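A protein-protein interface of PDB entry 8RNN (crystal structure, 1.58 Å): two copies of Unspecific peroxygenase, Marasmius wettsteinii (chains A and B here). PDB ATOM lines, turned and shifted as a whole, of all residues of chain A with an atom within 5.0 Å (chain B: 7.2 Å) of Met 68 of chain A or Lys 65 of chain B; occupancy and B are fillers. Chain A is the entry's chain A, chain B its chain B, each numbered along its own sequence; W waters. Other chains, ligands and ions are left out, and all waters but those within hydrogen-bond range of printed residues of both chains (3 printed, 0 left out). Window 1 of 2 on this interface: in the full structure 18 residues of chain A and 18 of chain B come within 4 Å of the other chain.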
ATOM      1  N   ILE A  40     -27.383  -1.285  -7.247  1.00  0.00           N
ATOM      2  CA  ILE A  40     -26.471  -0.759  -6.250  1.00  0.00           C
ATOM      3  C   ILE A  40     -25.115  -0.488  -6.899  1.00  0.00           C
ATOM      4  O   ILE A  40     -24.495  -1.389  -7.468  1.00  0.00           O
ATOM      5  CB  ILE A  40     -26.356  -1.718  -5.045  1.00  0.00           C
ATOM      6  CG1 ILE A  40     -27.655  -1.746  -4.239  1.00  0.00           C
ATOM      7  CG2 ILE A  40     -25.179  -1.391  -4.146  1.00  0.00           C
ATOM      8  CD1 ILE A  40     -27.749  -2.914  -3.286  1.00  0.00           C
ATOM      9  N   SER A  41     -24.642   0.753  -6.744  1.00  0.00           N
ATOM     10  CA  SER A  41     -23.371   1.205  -7.292  1.00  0.00           C
ATOM     11  C   SER A  41     -22.305   1.277  -6.201  1.00  0.00           C
ATOM     12  O   SER A  41     -22.595   1.245  -5.008  1.00  0.00           O
ATOM     13  CB  SER A  41     -23.557   2.557  -7.910  1.00  0.00           C
ATOM     14  OG  SER A  41     -23.772   3.527  -6.884  1.00  0.00           O
ATOM     15  N   VAL A  42     -21.041   1.472  -6.593  1.00  0.00           N
ATOM     16  CA  VAL A  42     -19.995   1.618  -5.602  1.00  0.00           C
ATOM     17  C   VAL A  42     -20.209   2.914  -4.817  1.00  0.00           C
ATOM     18  O   VAL A  42     -20.095   2.885  -3.605  1.00  0.00           O
ATOM     19  CB  VAL A  42     -18.581   1.495  -6.208  1.00  0.00           C
ATOM     20  CG1 VAL A  42     -17.492   1.767  -5.199  1.00  0.00           C
ATOM     21  CG2 VAL A  42     -18.368   0.111  -6.809  1.00  0.00           C
ATOM     22  N   ILE A  45     -22.583   2.101  -2.061  1.00  0.00           N
ATOM     23  CA  ILE A  45     -21.974   1.282  -1.028  1.00  0.00           C
ATOM     24  C   ILE A  45     -21.087   2.139  -0.117  1.00  0.00           C
ATOM     25  O   ILE A  45     -21.105   1.995   1.096  1.00  0.00           O
ATOM     26  CB  ILE A  45     -21.189   0.113  -1.665  1.00  0.00           C
ATOM     27  CG1 ILE A  45     -22.145  -0.882  -2.323  1.00  0.00           C
ATOM     28  CG2 ILE A  45     -20.289  -0.561  -0.646  1.00  0.00           C
ATOM     29  CD1 ILE A  45     -21.466  -1.895  -3.219  1.00  0.00           C
ATOM     30  N   GLY A  64     -15.650  -2.824  -3.444  1.00  0.00           N
ATOM     31  CA  GLY A  64     -16.820  -2.536  -4.242  1.00  0.00           C
ATOM     32  C   GLY A  64     -16.591  -2.762  -5.736  1.00  0.00           C
ATOM     33  O   GLY A  64     -17.430  -3.338  -6.423  1.00  0.00           O
ATOM     34  N   LYS A  65     -15.453  -2.269  -6.248  1.00  0.00           N
ATOM     35  CA  LYS A  65     -15.186  -2.399  -7.669  1.00  0.00           C
ATOM     36  C   LYS A  65     -14.913  -3.862  -8.037  1.00  0.00           C
ATOM     37  O   LYS A  65     -15.295  -4.266  -9.124  1.00  0.00           O
ATOM     38  CB  LYS A  65     -14.078  -1.433  -8.084  1.00  0.00           C
ATOM     39  CG  LYS A  65     -14.514   0.028  -8.084  1.00  0.00           C
ATOM     40  CD  LYS A  65     -13.497   0.954  -8.726  1.00  0.00           C
ATOM     41  CE  LYS A  65     -12.138   0.866  -8.078  1.00  0.00           C
ATOM     42  NZ  LYS A  65     -11.248   1.958  -8.545  1.00  0.00           N
ATOM     43  N   VAL A  66     -14.317  -4.652  -7.132  1.00  0.00           N
ATOM     44  CA  VAL A  66     -14.199  -6.084  -7.384  1.00  0.00           C
ATOM     45  C   VAL A  66     -15.599  -6.710  -7.421  1.00  0.00           C
ATOM     46  O   VAL A  66     -15.895  -7.536  -8.282  1.00  0.00           O
ATOM     47  CB  VAL A  66     -13.284  -6.781  -6.366  1.00  0.00           C
ATOM     48  CG1 VAL A  66     -13.264  -8.297  -6.572  1.00  0.00           C
ATOM     49  CG2 VAL A  66     -11.868  -6.227  -6.444  1.00  0.00           C
ATOM     50  N   GLY A  67     -16.469  -6.305  -6.491  1.00  0.00           N
ATOM     51  CA  GLY A  67     -17.830  -6.813  -6.454  1.00  0.00           C
ATOM     52  C   GLY A  67     -18.632  -6.488  -7.714  1.00  0.00           C
ATOM     53  O   GLY A  67     -19.465  -7.274  -8.152  1.00  0.00           O
ATOM     54  N   MET A  68     -18.395  -5.322  -8.327  1.00  0.00           N
ATOM     55  CA  MET A  68     -19.075  -4.944  -9.546  1.00  0.00           C
ATOM     56  C   MET A  68     -18.849  -5.973 -10.658  1.00  0.00           C
ATOM     57  O   MET A  68     -19.696  -6.100 -11.530  1.00  0.00           O
ATOM     58  CB  MET A  68     -18.613  -3.568 -10.038  1.00  0.00           C
ATOM     59  CG  MET A  68     -18.982  -2.396  -9.134  1.00  0.00           C
ATOM     60  SD  MET A  68     -20.778  -2.105  -8.931  1.00  0.00           S
ATOM     61  CE  MET A  68     -21.012  -2.522  -7.211  1.00  0.00           C
ATOM     62  N   LEU A  69     -17.713  -6.689 -10.631  1.00  0.00           N
ATOM     63  CA  LEU A  69     -17.417  -7.643 -11.688  1.00  0.00           C
ATOM     64  C   LEU A  69     -18.464  -8.760 -11.755  1.00  0.00           C
ATOM     65  O   LEU A  69     -18.607  -9.399 -12.802  1.00  0.00           O
ATOM     66  CB  LEU A  69     -16.033  -8.275 -11.490  1.00  0.00           C
ATOM     67  CG  LEU A  69     -14.845  -7.319 -11.403  1.00  0.00           C
ATOM     68  CD1 LEU A  69     -13.589  -8.068 -11.010  1.00  0.00           C
ATOM     69  CD2 LEU A  69     -14.626  -6.562 -12.712  1.00  0.00           C
ATOM     70  N   THR A  70     -19.215  -8.986 -10.664  1.00  0.00           N
ATOM     71  CA  THR A  70     -20.088 -10.157 -10.579  1.00  0.00           C
ATOM     72  C   THR A  70     -21.394  -9.983 -11.361  1.00  0.00           C
ATOM     73  O   THR A  70     -22.128 -10.951 -11.532  1.00  0.00           O
ATOM     74  CB  THR A  70     -20.399 -10.522  -9.122  1.00  0.00           C
ATOM     75  OG1 THR A  70     -21.191  -9.477  -8.526  1.00  0.00           O
ATOM     76  CG2 THR A  70     -19.145 -10.742  -8.296  1.00  0.00           C
ATOM     77  N   SER A  71     -21.723  -8.771 -11.817  1.00  0.00           N
ATOM     78  CA  SER A  71     -22.942  -8.542 -12.569  1.00  0.00           C
ATOM     79  C   SER A  71     -22.654  -8.385 -14.063  1.00  0.00           C
ATOM     80  O   SER A  71     -21.496  -8.259 -14.478  1.00  0.00           O
ATOM     81  CB  SER A  71     -23.654  -7.321 -12.059  1.00  0.00           C
ATOM     82  OG  SER A  71     -23.038  -6.150 -12.581  1.00  0.00           O
ATOM     83  N   ARG A  72     -23.743  -8.309 -14.846  1.00  0.00           N
ATOM     84  CA  ARG A  72     -23.678  -8.037 -16.273  1.00  0.00           C
ATOM     85  C   ARG A  72     -23.926  -6.556 -16.572  1.00  0.00           C
ATOM     86  O   ARG A  72     -23.954  -6.169 -17.740  1.00  0.00           O
ATOM     87  CB  ARG A  72     -24.699  -8.912 -17.009  1.00  0.00           C
ATOM     88  CG  ARG A  72     -24.347 -10.393 -16.988  1.00  0.00           C
ATOM     89  CD  ARG A  72     -25.336 -11.254 -17.753  1.00  0.00           C
ATOM     90  NE  ARG A  72     -24.779 -12.585 -17.975  1.00  0.00           N
ATOM     91  CZ  ARG A  72     -24.722 -13.545 -17.056  1.00  0.00           C
ATOM     92  NH1 ARG A  72     -25.352 -13.405 -15.902  1.00  0.00           N
ATOM     93  NH2 ARG A  72     -24.062 -14.664 -17.306  1.00  0.00           N
ATOM     94  N   GLU A  73     -24.097  -5.732 -15.529  1.00  0.00           N
ATOM     95  CA  GLU A  73     -24.425  -4.326 -15.743  1.00  0.00           C
ATOM     96  C   GLU A  73     -23.157  -3.470 -15.725  1.00  0.00           C
ATOM     97  O   GLU A  73     -22.133  -3.849 -15.158  1.00  0.00           O
ATOM     98  CB  GLU A  73     -25.445  -3.856 -14.704  1.00  0.00           C
ATOM     99  CG  GLU A  73     -26.850  -4.409 -14.923  1.00  0.00           C
ATOM    100  CD  GLU A  73     -27.030  -5.872 -14.566  1.00  0.00           C
ATOM    101  OE1 GLU A  73     -26.752  -6.233 -13.396  1.00  0.00           O
ATOM    102  OE2 GLU A  73     -27.460  -6.643 -15.454  1.00  0.00           O
ATOM    103  N   ALA A  74     -23.252  -2.286 -16.349  1.00  0.00           N
ATOM    104  CA  ALA A  74     -22.130  -1.367 -16.485  1.00  0.00           C
ATOM    105  C   ALA A  74     -21.565  -0.883 -15.145  1.00  0.00           C
ATOM    106  O   ALA A  74     -20.353  -0.736 -15.026  1.00  0.00           O
ATOM    107  CB  ALA A  74     -22.561  -0.183 -17.326  1.00  0.00           C
ATOM    108  N   ASP A  75     -22.413  -0.580 -14.148  1.00  0.00           N
ATOM    109  CA  ASP A  75     -21.908   0.024 -12.924  1.00  0.00           C
ATOM    110  C   ASP A  75     -22.753  -0.282 -11.688  1.00  0.00           C
ATOM    111  O   ASP A  75     -22.629   0.412 -10.683  1.00  0.00           O
ATOM    112  CB  ASP A  75     -21.741   1.543 -13.083  1.00  0.00           C
ATOM    113  CG  ASP A  75     -23.024   2.349 -13.248  1.00  0.00           C
ATOM    114  OD1 ASP A  75     -24.109   1.748 -13.351  1.00  0.00           O
ATOM    115  OD2 ASP A  75     -22.925   3.599 -13.218  1.00  0.00           O
ATOM    116  N   THR A  76     -23.550  -1.356 -11.730  1.00  0.00           N
ATOM    117  CA  THR A  76     -24.345  -1.743 -10.576  1.00  0.00           C
ATOM    118  C   THR A  76     -24.372  -3.259 -10.444  1.00  0.00           C
ATOM    119  O   THR A  76     -24.040  -3.974 -11.384  1.00  0.00           O
ATOM    120  CB  THR A  76     -25.800  -1.258 -10.657  1.00  0.00           C
ATOM    121  OG1 THR A  76     -26.436  -1.788 -11.815  1.00  0.00           O
ATOM    122  CG2 THR A  76     -25.917   0.246 -10.706  1.00  0.00           C
ATOM    123  N   ILE A  77     -24.781  -3.690  -9.251  1.00  0.00           N
ATOM    124  CA  ILE A  77     -25.047  -5.082  -8.935  1.00  0.00           C
ATOM    125  C   ILE A  77     -26.393  -5.200  -8.227  1.00  0.00           C
ATOM    126  O   ILE A  77     -26.930  -4.207  -7.726  1.00  0.00           O
ATOM    127  CB  ILE A  77     -23.963  -5.642  -7.994  1.00  0.00           C
ATOM    128  CG1 ILE A  77     -23.956  -4.944  -6.626  1.00  0.00           C
ATOM    129  CG2 ILE A  77     -22.612  -5.640  -8.683  1.00  0.00           C
ATOM    130  CD1 ILE A  77     -23.078  -5.584  -5.570  1.00  0.00           C
ATOM    131  N   VAL B  42     -17.667   3.487 -16.831  1.00  0.00           N
ATOM    132  CA  VAL B  42     -17.946   2.421 -17.771  1.00  0.00           C
ATOM    133  C   VAL B  42     -19.109   2.831 -18.679  1.00  0.00           C
ATOM    134  O   VAL B  42     -19.058   2.605 -19.874  1.00  0.00           O
ATOM    135  CB  VAL B  42     -18.160   1.076 -17.052  1.00  0.00           C
ATOM    136  CG1 VAL B  42     -18.610  -0.014 -18.012  1.00  0.00           C
ATOM    137  CG2 VAL B  42     -16.892   0.678 -16.300  1.00  0.00           C
ATOM    138  N   ILE B  45     -17.657   4.799 -21.469  1.00  0.00           N
ATOM    139  CA  ILE B  45     -16.901   3.967 -22.392  1.00  0.00           C
ATOM    140  C   ILE B  45     -17.851   3.197 -23.316  1.00  0.00           C
ATOM    141  O   ILE B  45     -17.629   3.124 -24.522  1.00  0.00           O
ATOM    142  CB  ILE B  45     -15.966   3.010 -21.621  1.00  0.00           C
ATOM    143  CG1 ILE B  45     -14.826   3.760 -20.931  1.00  0.00           C
ATOM    144  CG2 ILE B  45     -15.418   1.919 -22.531  1.00  0.00           C
ATOM    145  CD1 ILE B  45     -14.026   2.950 -19.922  1.00  0.00           C
ATOM    146  N   ILE B  59     -18.501  -6.523 -24.589  1.00  0.00           N
ATOM    147  CA  ILE B  59     -17.072  -6.476 -24.335  1.00  0.00           C
ATOM    148  C   ILE B  59     -16.706  -5.241 -23.506  1.00  0.00           C
ATOM    149  O   ILE B  59     -15.799  -5.311 -22.680  1.00  0.00           O
ATOM    150  CB  ILE B  59     -16.244  -6.581 -25.630  1.00  0.00           C
ATOM    151  CG1 ILE B  59     -14.747  -6.696 -25.331  1.00  0.00           C
ATOM    152  CG2 ILE B  59     -16.550  -5.425 -26.562  1.00  0.00           C
ATOM    153  CD1 ILE B  59     -13.913  -7.148 -26.515  1.00  0.00           C
ATOM    154  N   LEU B  60     -17.390  -4.107 -23.726  1.00  0.00           N
ATOM    155  CA  LEU B  60     -16.992  -2.873 -23.059  1.00  0.00           C
ATOM    156  C   LEU B  60     -17.375  -2.869 -21.575  1.00  0.00           C
ATOM    157  O   LEU B  60     -16.660  -2.281 -20.779  1.00  0.00           O
ATOM    158  CB  LEU B  60     -17.583  -1.678 -23.819  1.00  0.00           C
ATOM    159  CG  LEU B  60     -17.047  -1.505 -25.240  1.00  0.00           C
ATOM    160  CD1 LEU B  60     -17.731  -0.331 -25.946  1.00  0.00           C
ATOM    161  CD2 LEU B  60     -15.531  -1.330 -25.245  1.00  0.00           C
ATOM    162  N   ILE B  61     -18.473  -3.527 -21.189  1.00  0.00           N
ATOM    163  CA  ILE B  61     -18.795  -3.677 -19.776  1.00  0.00           C
ATOM    164  C   ILE B  61     -17.767  -4.575 -19.084  1.00  0.00           C
ATOM    165  O   ILE B  61     -17.290  -4.261 -17.987  1.00  0.00           O
ATOM    166  CB  ILE B  61     -20.242  -4.173 -19.598  1.00  0.00           C
ATOM    167  CG1 ILE B  61     -21.248  -3.074 -19.956  1.00  0.00           C
ATOM    168  CG2 ILE B  61     -20.469  -4.698 -18.188  1.00  0.00           C
ATOM    169  CD1 ILE B  61     -22.672  -3.531 -20.085  1.00  0.00           C
ATOM    170  N   LEU B  62     -17.465  -5.717 -19.718  1.00  0.00           N
ATOM    171  CA  LEU B  62     -16.538  -6.687 -19.158  1.00  0.00           C
ATOM    172  C   LEU B  62     -15.152  -6.068 -18.960  1.00  0.00           C
ATOM    173  O   LEU B  62     -14.620  -6.105 -17.847  1.00  0.00           O
ATOM    174  CB  LEU B  62     -16.516  -7.908 -20.080  1.00  0.00           C
ATOM    175  CG  LEU B  62     -15.595  -9.064 -19.700  1.00  0.00           C
ATOM    176  CD1 LEU B  62     -15.991  -9.685 -18.366  1.00  0.00           C
ATOM    177  CD2 LEU B  62     -15.642 -10.115 -20.794  1.00  0.00           C
ATOM    178  N   ALA B  63     -14.586  -5.478 -20.024  1.00  0.00           N
ATOM    179  CA  ALA B  63     -13.256  -4.885 -19.954  1.00  0.00           C
ATOM    180  C   ALA B  63     -13.273  -3.607 -19.113  1.00  0.00           C
ATOM    181  O   ALA B  63     -12.342  -3.342 -18.361  1.00  0.00           O
ATOM    182  CB  ALA B  63     -12.737  -4.616 -21.345  1.00  0.00           C
ATOM    183  N   GLY B  64     -14.344  -2.826 -19.250  1.00  0.00           N
ATOM    184  CA  GLY B  64     -14.458  -1.558 -18.558  1.00  0.00           C
ATOM    185  C   GLY B  64     -14.398  -1.706 -17.042  1.00  0.00           C
ATOM    186  O   GLY B  64     -13.711  -0.948 -16.364  1.00  0.00           O
ATOM    187  N   LYS B  65     -15.144  -2.681 -16.493  1.00  0.00           N
ATOM    188  CA  LYS B  65     -15.175  -2.852 -15.050  1.00  0.00           C
ATOM    189  C   LYS B  65     -13.833  -3.378 -14.537  1.00  0.00           C
ATOM    190  O   LYS B  65     -13.418  -3.010 -13.446  1.00  0.00           O
ATOM    191  CB  LYS B  65     -16.379  -3.698 -14.641  1.00  0.00           C
ATOM    192  CG  LYS B  65     -17.718  -2.999 -14.821  1.00  0.00           C
ATOM    193  CD  LYS B  65     -18.881  -3.738 -14.183  1.00  0.00           C
ATOM    194  CE  LYS B  65     -19.033  -5.143 -14.713  1.00  0.00           C
ATOM    195  NZ  LYS B  65     -20.313  -5.743 -14.270  1.00  0.00           N
ATOM    196  N   VAL B  66     -13.110  -4.197 -15.328  1.00  0.00           N
ATOM    197  CA  VAL B  66     -11.753  -4.570 -14.950  1.00  0.00           C
ATOM    198  C   VAL B  66     -10.856  -3.330 -14.949  1.00  0.00           C
ATOM    199  O   VAL B  66     -10.062  -3.133 -14.026  1.00  0.00           O
ATOM    200  CB  VAL B  66     -11.193  -5.692 -15.846  1.00  0.00           C
ATOM    201  CG1 VAL B  66      -9.729  -5.990 -15.545  1.00  0.00           C
ATOM    202  CG2 VAL B  66     -12.028  -6.959 -15.719  1.00  0.00           C
ATOM    203  N   GLY B  67     -11.022  -2.474 -15.963  1.00  0.00           N
ATOM    204  CA  GLY B  67     -10.250  -1.237 -16.049  1.00  0.00           C
ATOM    205  C   GLY B  67     -10.481  -0.298 -14.864  1.00  0.00           C
ATOM    206  O   GLY B  67      -9.557   0.374 -14.398  1.00  0.00           O
ATOM    207  N   MET B  68     -11.708  -0.277 -14.340  1.00  0.00           N
ATOM    208  CA  MET B  68     -12.012   0.569 -13.196  1.00  0.00           C
ATOM    209  C   MET B  68     -11.144   0.232 -11.980  1.00  0.00           C
ATOM    210  O   MET B  68     -10.909   1.098 -11.147  1.00  0.00           O
ATOM    211  CB  MET B  68     -13.491   0.464 -12.800  1.00  0.00           C
ATOM    212  CG  MET B  68     -14.471   0.949 -13.832  1.00  0.00           C
ATOM    213  SD  MET B  68     -14.362   2.747 -14.161  1.00  0.00           S
ATOM    214  CE  MET B  68     -13.783   2.772 -15.856  1.00  0.00           C
ATOM    215  N   LEU B  69     -10.657  -1.015 -11.864  1.00  0.00           N
ATOM    216  CA  LEU B  69      -9.858  -1.411 -10.708  1.00  0.00           C
ATOM    217  C   LEU B  69      -8.570  -0.592 -10.605  1.00  0.00           C
ATOM    218  O   LEU B  69      -7.981  -0.514  -9.533  1.00  0.00           O
ATOM    219  CB  LEU B  69      -9.516  -2.904 -10.786  1.00  0.00           C
ATOM    220  CG  LEU B  69     -10.699  -3.873 -10.886  1.00  0.00           C
ATOM    221  CD1 LEU B  69     -10.191  -5.277 -11.155  1.00  0.00           C
ATOM    222  CD2 LEU B  69     -11.542  -3.880  -9.618  1.00  0.00           C
ATOM    223  N   THR B  70      -8.120   0.001 -11.723  1.00  0.00           N
ATOM    224  CA  THR B  70      -6.795   0.610 -11.768  1.00  0.00           C
ATOM    225  C   THR B  70      -6.746   1.980 -11.086  1.00  0.00           C
ATOM    226  O   THR B  70      -5.651   2.498 -10.880  1.00  0.00           O
ATOM    227  CB  THR B  70      -6.279   0.732 -13.210  1.00  0.00           C
ATOM    228  OG1 THR B  70      -7.081   1.648 -13.949  1.00  0.00           O
ATOM    229  CG2 THR B  70      -6.260  -0.591 -13.941  1.00  0.00           C
ATOM    230  N   ALA B  74     -14.296   5.773  -7.077  1.00  0.00           N
ATOM    231  CA  ALA B  74     -15.380   4.813  -6.873  1.00  0.00           C
ATOM    232  C   ALA B  74     -15.863   4.208  -8.192  1.00  0.00           C
ATOM    233  O   ALA B  74     -16.222   3.033  -8.227  1.00  0.00           O
ATOM    234  CB  ALA B  74     -16.531   5.459  -6.143  1.00  0.00           C
ATOM    235  N   THR B  87      -3.050  -5.539 -14.248  1.00  0.00           N
ATOM    236  CA  THR B  87      -4.506  -5.551 -14.260  1.00  0.00           C
ATOM    237  C   THR B  87      -4.921  -5.967 -15.672  1.00  0.00           C
ATOM    238  O   THR B  87      -5.188  -7.143 -15.905  1.00  0.00           O
ATOM    239  CB  THR B  87      -5.122  -4.238 -13.743  1.00  0.00           C
ATOM    240  OG1 THR B  87      -4.690  -3.998 -12.402  1.00  0.00           O
ATOM    241  CG2 THR B  87      -6.637  -4.260 -13.758  1.00  0.00           C
ATOM    242  N   ILE B  88      -4.905  -5.023 -16.622  1.00  0.00           N
ATOM    243  CA  ILE B  88      -5.026  -5.325 -18.046  1.00  0.00           C
ATOM    244  C   ILE B  88      -3.658  -5.187 -18.710  1.00  0.00           C
ATOM    245  O   ILE B  88      -3.267  -6.042 -19.508  1.00  0.00           O
ATOM    246  CB  ILE B  88      -6.082  -4.432 -18.723  1.00  0.00           C
ATOM    247  CG1 ILE B  88      -7.467  -4.677 -18.117  1.00  0.00           C
ATOM    248  CG2 ILE B  88      -6.074  -4.627 -20.233  1.00  0.00           C
ATOM    249  CD1 ILE B  88      -8.505  -3.672 -18.534  1.00  0.00           C
HETATM  250  O   HOH W   1      -9.290   0.097  -6.977  1.00  0.00           O
HETATM  251  O   HOH W   2     -15.200  -2.637 -11.357  1.00  0.00           O
HETATM  252  O   HOH W   3     -18.673  -8.107 -15.513  1.00  0.00           O
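Val 42 of chain A touches Ala 74 of chain B, and with the chains exchanged Ala 74 of chain A touches Val 42 of chain B. Lys 65 of chain A touches Leu 69 of chain B, and with the chains exchanged Leu 69 of chain A touches Lys 65 of chain B. Lys 65 of chain A touches Ala 74 of chain B, and with the chains exchanged Ala 74 of chain A touches Lys 65 of chain B. Val 66 of chain A touches Leu 69 of chain B, and with the chains exchanged Leu 69 of chain A touches Val 66 of chain B.
No residue of chain B comes within 4 Å of Gly 67 of chain A. Printed residues of chain A within 4 Å of Ile 61 of chain B: Arg 72, Glu 73 and Ala 74. Lys 65 of chain B touches just these residues of chain A: Met 68 (2.8 Å), Leu 69 (3.8 Å), Ser 71 (2.8 Å), Glu 73 (2.8 Å) and Ala 74 (3.4 Å). Of the printed residues of chain A, Leu 69 of chain B touches Lys 65 and Val 66. Thr 70 of chain B touches none of the printed residues of chain A. Thr 87 of chain B touches none of the printed residues of chain A.
Printed residues of chain A that touch a printed residue of chain B: Val 42, Lys 65, Val 66, Met 68, Leu 69, Ser 71, Arg 72, Glu 73 and Ala 74. Hydrophobic or aromatic side chains of chain B that line the printed part of chain A: Val 42, Ile 61, Val 66, Leu 69 and Ala 74.
Water W2 bridges the backbone carbonyl oxygen of Lys 65 of chain A and the backbone carbonyl oxygen of Lys 65 of chain B. Water W1 lies within hydrogen-bond range of O of Leu 69 of chain B (2.9 Å) and NZ of Lys 65 of chain A (3.1 Å). Water W3 lies within hydrogen-bond range of the backbone carbonyl oxygen of Leu 69 of chain A (3.0 Å), the backbone carbonyl oxygen of Ser 71 of chain A (3.0 Å) and the side-chain amino group of Lys 65 of chain B (3.1 Å).
OG of Ser 71 of chain A sits at hydrogen-bond distance from N of Glu 73 of chain A (3.2 Å). The side-chain hydroxyl (OG) of Ser 71 of chain A lies within hydrogen-bond range of the backbone carbonyl oxygen (O) of Thr 76 of chain A, at 2.7 Å.
The side-chain amino group of Lys 65 of chain A lies within hydrogen-bond range of the backbone carbonyl oxygen of Met 68 of chain B. O of Met 68 of chain A is in hydrogen-bond range of NZ of Lys 65 of chain B, at 2.8 Å. NZ of Lys 65 of chain B lies within hydrogen-bond range of O of Ser 71 of chain A, 2.8 Å away. O of Glu 73 of chain A is in hydrogen-bond range of NZ of Lys 65 of chain B (2.8 Å).
CB of Val 42 of chain A touches O of Ala 74 of chain B, 3.5 Å away. CD2 of Leu 69 of chain B touches C of Lys 65 of chain A, 3.7 Å away. Ala 74 of chain B touches Lys 65 of chain A. CD2 of Leu 69 of chain B touches N of Val 66 of chain A (3.8 Å). C of Lys 65 of chain B touches CD2 of Leu 69 of chain A, at 3.8 Å. Leu 69 of chain A touches Val 66 of chain B (CD2 to N, 3.8 Å). O of Arg 72 of chain A touches CD1 of Ile 61 of chain B (3.8 Å). Ala 74 of chain A touches Val 42 of chain B. Ala 74 of chain A touches Ile 61 of chain B (CA to CG1, 3.97 Å). CD of Lys 65 of chain B touches O of Ala 74 of chain A, at 3.4 Å.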
